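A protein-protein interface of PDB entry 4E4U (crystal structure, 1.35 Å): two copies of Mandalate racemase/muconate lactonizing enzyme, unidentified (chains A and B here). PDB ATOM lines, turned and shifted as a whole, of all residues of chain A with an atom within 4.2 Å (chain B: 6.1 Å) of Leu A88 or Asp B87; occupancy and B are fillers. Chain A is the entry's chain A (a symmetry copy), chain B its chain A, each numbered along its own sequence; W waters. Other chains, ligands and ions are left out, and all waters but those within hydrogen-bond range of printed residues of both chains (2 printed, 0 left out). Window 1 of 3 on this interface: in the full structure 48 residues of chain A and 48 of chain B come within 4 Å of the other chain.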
ATOM      1  N   THR A  44      31.021 -13.810  21.190  1.00  0.00           N
ATOM      2  CA  THR A  44      30.205 -12.862  20.437  1.00  0.00           C
ATOM      3  C   THR A  44      30.994 -11.571  20.209  1.00  0.00           C
ATOM      4  O   THR A  44      30.989 -11.011  19.102  1.00  0.00           O
ATOM      5  CB  THR A  44      28.912 -12.539  21.186  1.00  0.00           C
ATOM      6  OG1 THR A  44      28.238 -13.757  21.514  1.00  0.00           O
ATOM      7  CG2 THR A  44      27.995 -11.677  20.335  1.00  0.00           C
ATOM      8  N   PHE A  45      31.669 -11.122  21.272  1.00  0.00           N
ATOM      9  CA  PHE A  45      32.511  -9.928  21.257  1.00  0.00           C
ATOM     10  C   PHE A  45      33.929 -10.332  21.607  1.00  0.00           C
ATOM     11  O   PHE A  45      34.130 -11.313  22.327  1.00  0.00           O
ATOM     12  CB  PHE A  45      32.024  -8.896  22.280  1.00  0.00           C
ATOM     13  CG  PHE A  45      30.543  -8.693  22.266  1.00  0.00           C
ATOM     14  CD1 PHE A  45      29.913  -8.180  21.139  1.00  0.00           C
ATOM     15  CD2 PHE A  45      29.771  -9.024  23.371  1.00  0.00           C
ATOM     16  CE1 PHE A  45      28.532  -8.002  21.117  1.00  0.00           C
ATOM     17  CE2 PHE A  45      28.393  -8.852  23.351  1.00  0.00           C
ATOM     18  CZ  PHE A  45      27.771  -8.337  22.221  1.00  0.00           C
ATOM     19  N   PRO A  86      17.691 -15.681  28.301  1.00  0.00           N
ATOM     20  CA  PRO A  86      19.140 -15.856  28.142  1.00  0.00           C
ATOM     21  C   PRO A  86      19.824 -14.753  27.330  1.00  0.00           C
ATOM     22  O   PRO A  86      19.392 -14.462  26.210  1.00  0.00           O
ATOM     23  CB  PRO A  86      19.248 -17.198  27.412  1.00  0.00           C
ATOM     24  CG  PRO A  86      18.015 -17.939  27.838  1.00  0.00           C
ATOM     25  CD  PRO A  86      16.938 -16.875  27.885  1.00  0.00           C
ATOM     26  N   ASP A  87      20.861 -14.147  27.911  1.00  0.00           N
ATOM     27  CA  ASP A  87      21.797 -13.292  27.192  1.00  0.00           C
ATOM     28  C   ASP A  87      23.088 -14.103  27.092  1.00  0.00           C
ATOM     29  O   ASP A  87      23.732 -14.392  28.102  1.00  0.00           O
ATOM     30  CB  ASP A  87      22.017 -11.962  27.928  1.00  0.00           C
ATOM     31  CG  ASP A  87      23.062 -11.079  27.243  1.00  0.00           C
ATOM     32  OD1 ASP A  87      24.211 -11.553  27.054  1.00  0.00           O
ATOM     33  OD2 ASP A  87      22.743  -9.911  26.903  1.00  0.00           O
ATOM     34  N   LEU A  88      23.442 -14.491  25.873  1.00  0.00           N
ATOM     35  CA  LEU A  88      24.494 -15.482  25.661  1.00  0.00           C
ATOM     36  C   LEU A  88      25.841 -15.085  26.288  1.00  0.00           C
ATOM     37  O   LEU A  88      26.507 -15.907  26.921  1.00  0.00           O
ATOM     38  CB  LEU A  88      24.661 -15.736  24.162  1.00  0.00           C
ATOM     39  CG  LEU A  88      25.635 -16.840  23.757  1.00  0.00           C
ATOM     40  CD1 LEU A  88      25.135 -18.214  24.192  1.00  0.00           C
ATOM     41  CD2 LEU A  88      25.848 -16.801  22.260  1.00  0.00           C
ATOM     42  N   THR A  89      26.248 -13.831  26.119  1.00  0.00           N
ATOM     43  CA  THR A  89      27.518 -13.399  26.693  1.00  0.00           C
ATOM     44  C   THR A  89      27.440 -13.367  28.212  1.00  0.00           C
ATOM     45  O   THR A  89      28.372 -13.814  28.889  1.00  0.00           O
ATOM     46  CB  THR A  89      27.975 -12.038  26.129  1.00  0.00           C
ATOM     47  OG1 THR A  89      28.212 -12.166  24.722  1.00  0.00           O
ATOM     48  CG2 THR A  89      29.249 -11.564  26.806  1.00  0.00           C
ATOM     49  N   MET A  90      26.325 -12.879  28.753  1.00  0.00           N
ATOM     50  CA  MET A  90      26.162 -12.835  30.207  1.00  0.00           C
ATOM     51  C   MET A  90      26.225 -14.238  30.786  1.00  0.00           C
ATOM     52  O   MET A  90      26.826 -14.456  31.833  1.00  0.00           O
ATOM     53  CB  MET A  90      24.834 -12.182  30.590  1.00  0.00           C
ATOM     54  CG  MET A  90      24.505 -12.279  32.080  1.00  0.00           C
ATOM     55  SD  MET A  90      25.732 -11.496  33.158  1.00  0.00           S
ATOM     56  CE  MET A  90      24.931  -9.919  33.444  1.00  0.00           C
ATOM     57  N   MET A  91      25.612 -15.199  30.105  1.00  0.00           N
ATOM     58  CA  MET A  91      25.636 -16.561  30.602  1.00  0.00           C
ATOM     59  C   MET A  91      27.048 -17.143  30.600  1.00  0.00           C
ATOM     60  O   MET A  91      27.426 -17.854  31.532  1.00  0.00           O
ATOM     61  CB  MET A  91      24.656 -17.433  29.837  1.00  0.00           C
ATOM     62  CG  MET A  91      23.192 -17.100  30.126  1.00  0.00           C
ATOM     63  SD  MET A  91      22.687 -17.370  31.840  1.00  0.00           S
ATOM     64  CE  MET A  91      22.883 -15.748  32.575  1.00  0.00           C
ATOM     65  N   GLY A  92      27.841 -16.839  29.573  1.00  0.00           N
ATOM     66  CA  GLY A  92      29.243 -17.234  29.586  1.00  0.00           C
ATOM     67  C   GLY A  92      29.988 -16.631  30.766  1.00  0.00           C
ATOM     68  O   GLY A  92      30.724 -17.319  31.477  1.00  0.00           O
ATOM     69  N   THR A 262      22.354 -22.220  25.869  1.00  0.00           N
ATOM     70  CA  THR A 262      22.648 -21.793  27.223  1.00  0.00           C
ATOM     71  C   THR A 262      21.389 -21.810  28.083  1.00  0.00           C
ATOM     72  O   THR A 262      20.296 -21.505  27.601  1.00  0.00           O
ATOM     73  CB  THR A 262      23.302 -20.390  27.243  1.00  0.00           C
ATOM     74  OG1 THR A 262      23.652 -20.056  28.590  1.00  0.00           O
ATOM     75  CG2 THR A 262      22.371 -19.325  26.648  1.00  0.00           C
ATOM     76  N   ARG A 285      29.607 -21.971  29.328  1.00  0.00           N
ATOM     77  CA  ARG A 285      28.606 -21.186  28.597  1.00  0.00           C
ATOM     78  C   ARG A 285      27.195 -21.282  29.180  1.00  0.00           C
ATOM     79  O   ARG A 285      26.431 -20.317  29.107  1.00  0.00           O
ATOM     80  CB  ARG A 285      28.562 -21.606  27.118  1.00  0.00           C
ATOM     81  CG  ARG A 285      27.293 -21.181  26.372  1.00  0.00           C
ATOM     82  CD  ARG A 285      27.464 -21.313  24.881  1.00  0.00           C
ATOM     83  NE  ARG A 285      28.146 -20.146  24.333  1.00  0.00           N
ATOM     84  CZ  ARG A 285      28.782 -20.103  23.167  1.00  0.00           C
ATOM     85  NH1 ARG A 285      28.888 -21.190  22.404  1.00  0.00           N
ATOM     86  NH2 ARG A 285      29.322 -18.960  22.767  1.00  0.00           N
ATOM     87  N   TYR B  78      24.725 -11.578  13.860  1.00  0.00           N
ATOM     88  CA  TYR B  78      24.018 -12.733  14.397  1.00  0.00           C
ATOM     89  C   TYR B  78      24.918 -13.962  14.512  1.00  0.00           C
ATOM     90  O   TYR B  78      24.719 -14.801  15.385  1.00  0.00           O
ATOM     91  CB  TYR B  78      22.808 -13.025  13.494  1.00  0.00           C
ATOM     92  CG  TYR B  78      21.907 -14.155  13.937  1.00  0.00           C
ATOM     93  CD1 TYR B  78      21.111 -14.035  15.066  1.00  0.00           C
ATOM     94  CD2 TYR B  78      21.827 -15.329  13.203  1.00  0.00           C
ATOM     95  CE1 TYR B  78      20.269 -15.050  15.456  1.00  0.00           C
ATOM     96  CE2 TYR B  78      20.992 -16.360  13.591  1.00  0.00           C
ATOM     97  CZ  TYR B  78      20.214 -16.217  14.723  1.00  0.00           C
ATOM     98  OH  TYR B  78      19.367 -17.224  15.134  1.00  0.00           O
ATOM     99  N   THR B  83      28.250 -18.149  16.779  1.00  0.00           N
ATOM    100  CA  THR B  83      27.040 -18.140  17.585  1.00  0.00           C
ATOM    101  C   THR B  83      25.860 -18.521  16.688  1.00  0.00           C
ATOM    102  O   THR B  83      25.486 -19.692  16.628  1.00  0.00           O
ATOM    103  CB  THR B  83      26.870 -16.786  18.333  1.00  0.00           C
ATOM    104  OG1 THR B  83      26.957 -15.697  17.404  1.00  0.00           O
ATOM    105  CG2 THR B  83      27.964 -16.638  19.409  1.00  0.00           C
ATOM    106  N   ARG B  85      22.812 -17.868  16.957  1.00  0.00           N
ATOM    107  CA  ARG B  85      21.538 -17.862  17.670  1.00  0.00           C
ATOM    108  C   ARG B  85      21.524 -16.524  18.402  1.00  0.00           C
ATOM    109  O   ARG B  85      22.563 -15.885  18.515  1.00  0.00           O
ATOM    110  CB  ARG B  85      21.367 -19.078  18.610  1.00  0.00           C
ATOM    111  CG  ARG B  85      22.621 -19.553  19.362  1.00  0.00           C
ATOM    112  CD  ARG B  85      23.192 -18.558  20.394  1.00  0.00           C
ATOM    113  NE  ARG B  85      22.150 -17.963  21.233  1.00  0.00           N
ATOM    114  CZ  ARG B  85      21.519 -18.575  22.235  1.00  0.00           C
ATOM    115  NH1 ARG B  85      21.846 -19.812  22.589  1.00  0.00           N
ATOM    116  NH2 ARG B  85      20.565 -17.934  22.901  1.00  0.00           N
ATOM    117  N   PRO B  86      20.360 -16.082  18.881  1.00  0.00           N
ATOM    118  CA  PRO B  86      20.331 -14.705  19.392  1.00  0.00           C
ATOM    119  C   PRO B  86      21.241 -14.459  20.598  1.00  0.00           C
ATOM    120  O   PRO B  86      21.152 -15.191  21.589  1.00  0.00           O
ATOM    121  CB  PRO B  86      18.863 -14.514  19.785  1.00  0.00           C
ATOM    122  CG  PRO B  86      18.122 -15.444  18.871  1.00  0.00           C
ATOM    123  CD  PRO B  86      19.013 -16.665  18.778  1.00  0.00           C
ATOM    124  N   ASP B  87      22.109 -13.452  20.488  1.00  0.00           N
ATOM    125  CA  ASP B  87      22.840 -12.896  21.620  1.00  0.00           C
ATOM    126  C   ASP B  87      22.202 -11.533  21.882  1.00  0.00           C
ATOM    127  O   ASP B  87      22.288 -10.625  21.052  1.00  0.00           O
ATOM    128  CB  ASP B  87      24.340 -12.771  21.309  1.00  0.00           C
ATOM    129  CG  ASP B  87      25.120 -12.108  22.446  1.00  0.00           C
ATOM    130  OD1 ASP B  87      24.760 -10.967  22.830  1.00  0.00           O
ATOM    131  OD2 ASP B  87      26.098 -12.719  22.949  1.00  0.00           O
ATOM    132  N   LEU B  88      21.537 -11.407  23.024  1.00  0.00           N
ATOM    133  CA  LEU B  88      20.666 -10.264  23.281  1.00  0.00           C
ATOM    134  C   LEU B  88      21.387  -8.910  23.165  1.00  0.00           C
ATOM    135  O   LEU B  88      20.864  -7.968  22.568  1.00  0.00           O
ATOM    136  CB  LEU B  88      20.028 -10.409  24.662  1.00  0.00           C
ATOM    137  CG  LEU B  88      18.986  -9.362  25.051  1.00  0.00           C
ATOM    138  CD1 LEU B  88      17.736  -9.470  24.182  1.00  0.00           C
ATOM    139  CD2 LEU B  88      18.633  -9.519  26.513  1.00  0.00           C
ATOM    140  N   THR B  89      22.586  -8.806  23.730  1.00  0.00           N
ATOM    141  CA  THR B  89      23.315  -7.545  23.652  1.00  0.00           C
ATOM    142  C   THR B  89      23.758  -7.267  22.223  1.00  0.00           C
ATOM    143  O   THR B  89      23.638  -6.133  21.747  1.00  0.00           O
ATOM    144  CB  THR B  89      24.511  -7.507  24.624  1.00  0.00           C
ATOM    145  OG1 THR B  89      24.028  -7.587  25.971  1.00  0.00           O
ATOM    146  CG2 THR B  89      25.311  -6.225  24.461  1.00  0.00           C
ATOM    147  N   MET B  90      24.235  -8.296  21.524  1.00  0.00           N
ATOM    148  CA  MET B  90      24.661  -8.118  20.135  1.00  0.00           C
ATOM    149  C   MET B  90      23.494  -7.649  19.283  1.00  0.00           C
ATOM    150  O   MET B  90      23.653  -6.787  18.424  1.00  0.00           O
ATOM    151  CB  MET B  90      25.223  -9.418  19.563  1.00  0.00           C
ATOM    152  CG  MET B  90      25.504  -9.362  18.061  1.00  0.00           C
ATOM    153  SD  MET B  90      26.703  -8.092  17.583  1.00  0.00           S
ATOM    154  CE  MET B  90      28.185  -9.093  17.465  1.00  0.00           C
ATOM    155  N   MET B  91      22.313  -8.207  19.520  1.00  0.00           N
ATOM    156  CA  MET B  91      21.157  -7.802  18.744  1.00  0.00           C
ATOM    157  C   MET B  91      20.779  -6.346  19.001  1.00  0.00           C
ATOM    158  O   MET B  91      20.409  -5.629  18.071  1.00  0.00           O
ATOM    159  CB  MET B  91      19.991  -8.747  18.978  1.00  0.00           C
ATOM    160  CG  MET B  91      20.205 -10.138  18.379  1.00  0.00           C
ATOM    161  SD  MET B  91      20.362 -10.162  16.578  1.00  0.00           S
ATOM    162  CE  MET B  91      22.136 -10.117  16.331  1.00  0.00           C
ATOM    163  N   GLY B  92      20.881  -5.891  20.249  1.00  0.00           N
ATOM    164  CA  GLY B  92      20.684  -4.477  20.534  1.00  0.00           C
ATOM    165  C   GLY B  92      21.680  -3.606  19.785  1.00  0.00           C
ATOM    166  O   GLY B  92      21.315  -2.604  19.167  1.00  0.00           O
ATOM    167  N   THR B 262      14.040 -10.946  20.903  1.00  0.00           N
ATOM    168  CA  THR B 262      14.860 -10.429  19.825  1.00  0.00           C
ATOM    169  C   THR B 262      14.926 -11.422  18.670  1.00  0.00           C
ATOM    170  O   THR B 262      14.945 -12.636  18.887  1.00  0.00           O
ATOM    171  CB  THR B 262      16.283 -10.074  20.319  1.00  0.00           C
ATOM    172  OG1 THR B 262      17.020  -9.488  19.240  1.00  0.00           O
ATOM    173  CG2 THR B 262      17.015 -11.308  20.865  1.00  0.00           C
HETATM  174  O   HOH W   1      21.118 -14.109  24.109  1.00  0.00           O
HETATM  175  O   HOH W   2      25.637 -10.285  25.227  1.00  0.00           O
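Among the printed residues, merely in contact across the chains: Leu A88 with Thr B83 (3.6 Å), Leu A88 with Asp B87 (3.6 Å), Asp A87 with Leu B88 (3.6 Å), Thr A44 with Thr B83 (3.6 Å), Phe A45 with Met B90 (3.6 Å), Thr A44 with Met B90 (3.7 Å), Leu A88 with Arg B85 (3.7 Å) and Phe A45 with Thr B89 (3.9 Å).
The side-chain carboxylate (OD2) of Asp B87 lies within hydrogen-bond range of the side-chain hydroxyl (OG1) of Thr A44 (2.8 Å). OD2 of Asp B87 sits at hydrogen-bond distance from OG1 of Thr A89, at 2.8 Å. OG1 of Thr B89 is in hydrogen-bond range of OD2 of Asp A87 (2.8 Å).
Asp A87 touches Leu B88, and with the chains exchanged Leu A88 touches Asp B87. Asp A87 touches Thr B89, and with the chains exchanged Thr A89 touches Asp B87. Of the 11 pairs that touch across the chains among the printed residues, 4 have their exchanged pair printed and touching as well.
Water W2 lies within hydrogen-bond range of OD1 of Asp A87 (2.6 Å), OD1 of Asp B87 (2.6 Å), OG1 of Thr B89 (3.2 Å) and OG1 of Thr A89 (3.2 Å). Water W1 lies within hydrogen-bond range of O of Pro A86 (2.7 Å), O of Pro B86 (2.7 Å), N of Leu B88 (2.9 Å) and N of Leu A88 (2.9 Å).
Of the 11 printed residues of chain A, 5 touch a printed residue of chain B. Printed residues of chain A that touch a printed residue of chain B: Thr A44, Phe A45, Asp A87, Leu A88 and Thr A89. Hydrophobic or aromatic side chains of chain A within 4 Å of the printed part of chain B: Phe A45 and Leu A88. Along chain A the printed residues that touch a printed residue of chain B span positions 44 to 89. Of the 11 printed residues of chain B, 6 touch a printed residue of chain A. Hydrophobic or aromatic side chains of chain B within 4 Å of the printed part of chain A: Leu B88 and Met B90. Along chain B the printed residues that touch a printed residue of chain A span positions 83 to 90. Among the printed residues, 11 pairs touch across the chains. Among the printed residues, no Asp or Glu carboxylate lies within 4 Å of a Lys or Arg side-chain nitrogen of the other chain.
The backbone carbonyl oxygen of Tyr B78 lies within hydrogen-bond range of the side-chain hydroxyl of Thr B83 (3.1 Å). The side-chain carboxylate (OD1) of Asp B87 lies within hydrogen-bond range of the backbone NH (N) of Thr B89. The side-chain carboxylate (OD1) of Asp B87 sits at hydrogen-bond distance from the backbone NH (N) of Met B90 (3.0 Å). The side-chain carboxylate (OD1) of Asp A87 is in hydrogen-bond range of the backbone NH (N) of Thr A89, at 3.2 Å. The side-chain carboxylate (OD1) of Asp A87 is in hydrogen-bond range of the backbone NH (N) of Met A90.
Leu A88 touches just these residues of chain B: Thr B83 (3.6 Å), Arg B85 (3.7 Å) and Asp B87 (3.6 Å). Of the printed residues of chain A, Thr B83 touches Thr A44 and Leu A88. Printed residues of chain B within 4 Å of Phe A45: Thr B89 and Met B90. Of the printed residues of chain B, Asp A87 touches Leu B88 (3.6 Å) and Thr B89 (2.8 Å). Printed residues of chain A within 4 Å of Thr B89: Phe A45 and Asp A87. Of the printed residues of chain A, Leu B88 touches Asp A87 (3.6 Å). Pro B86 touches none of the printed residues of chain A. Thr A262 touches none of the printed residues of chain B. The nearest residue of chain B that does not touch Leu A88 is Pro B86 (4.4 Å).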
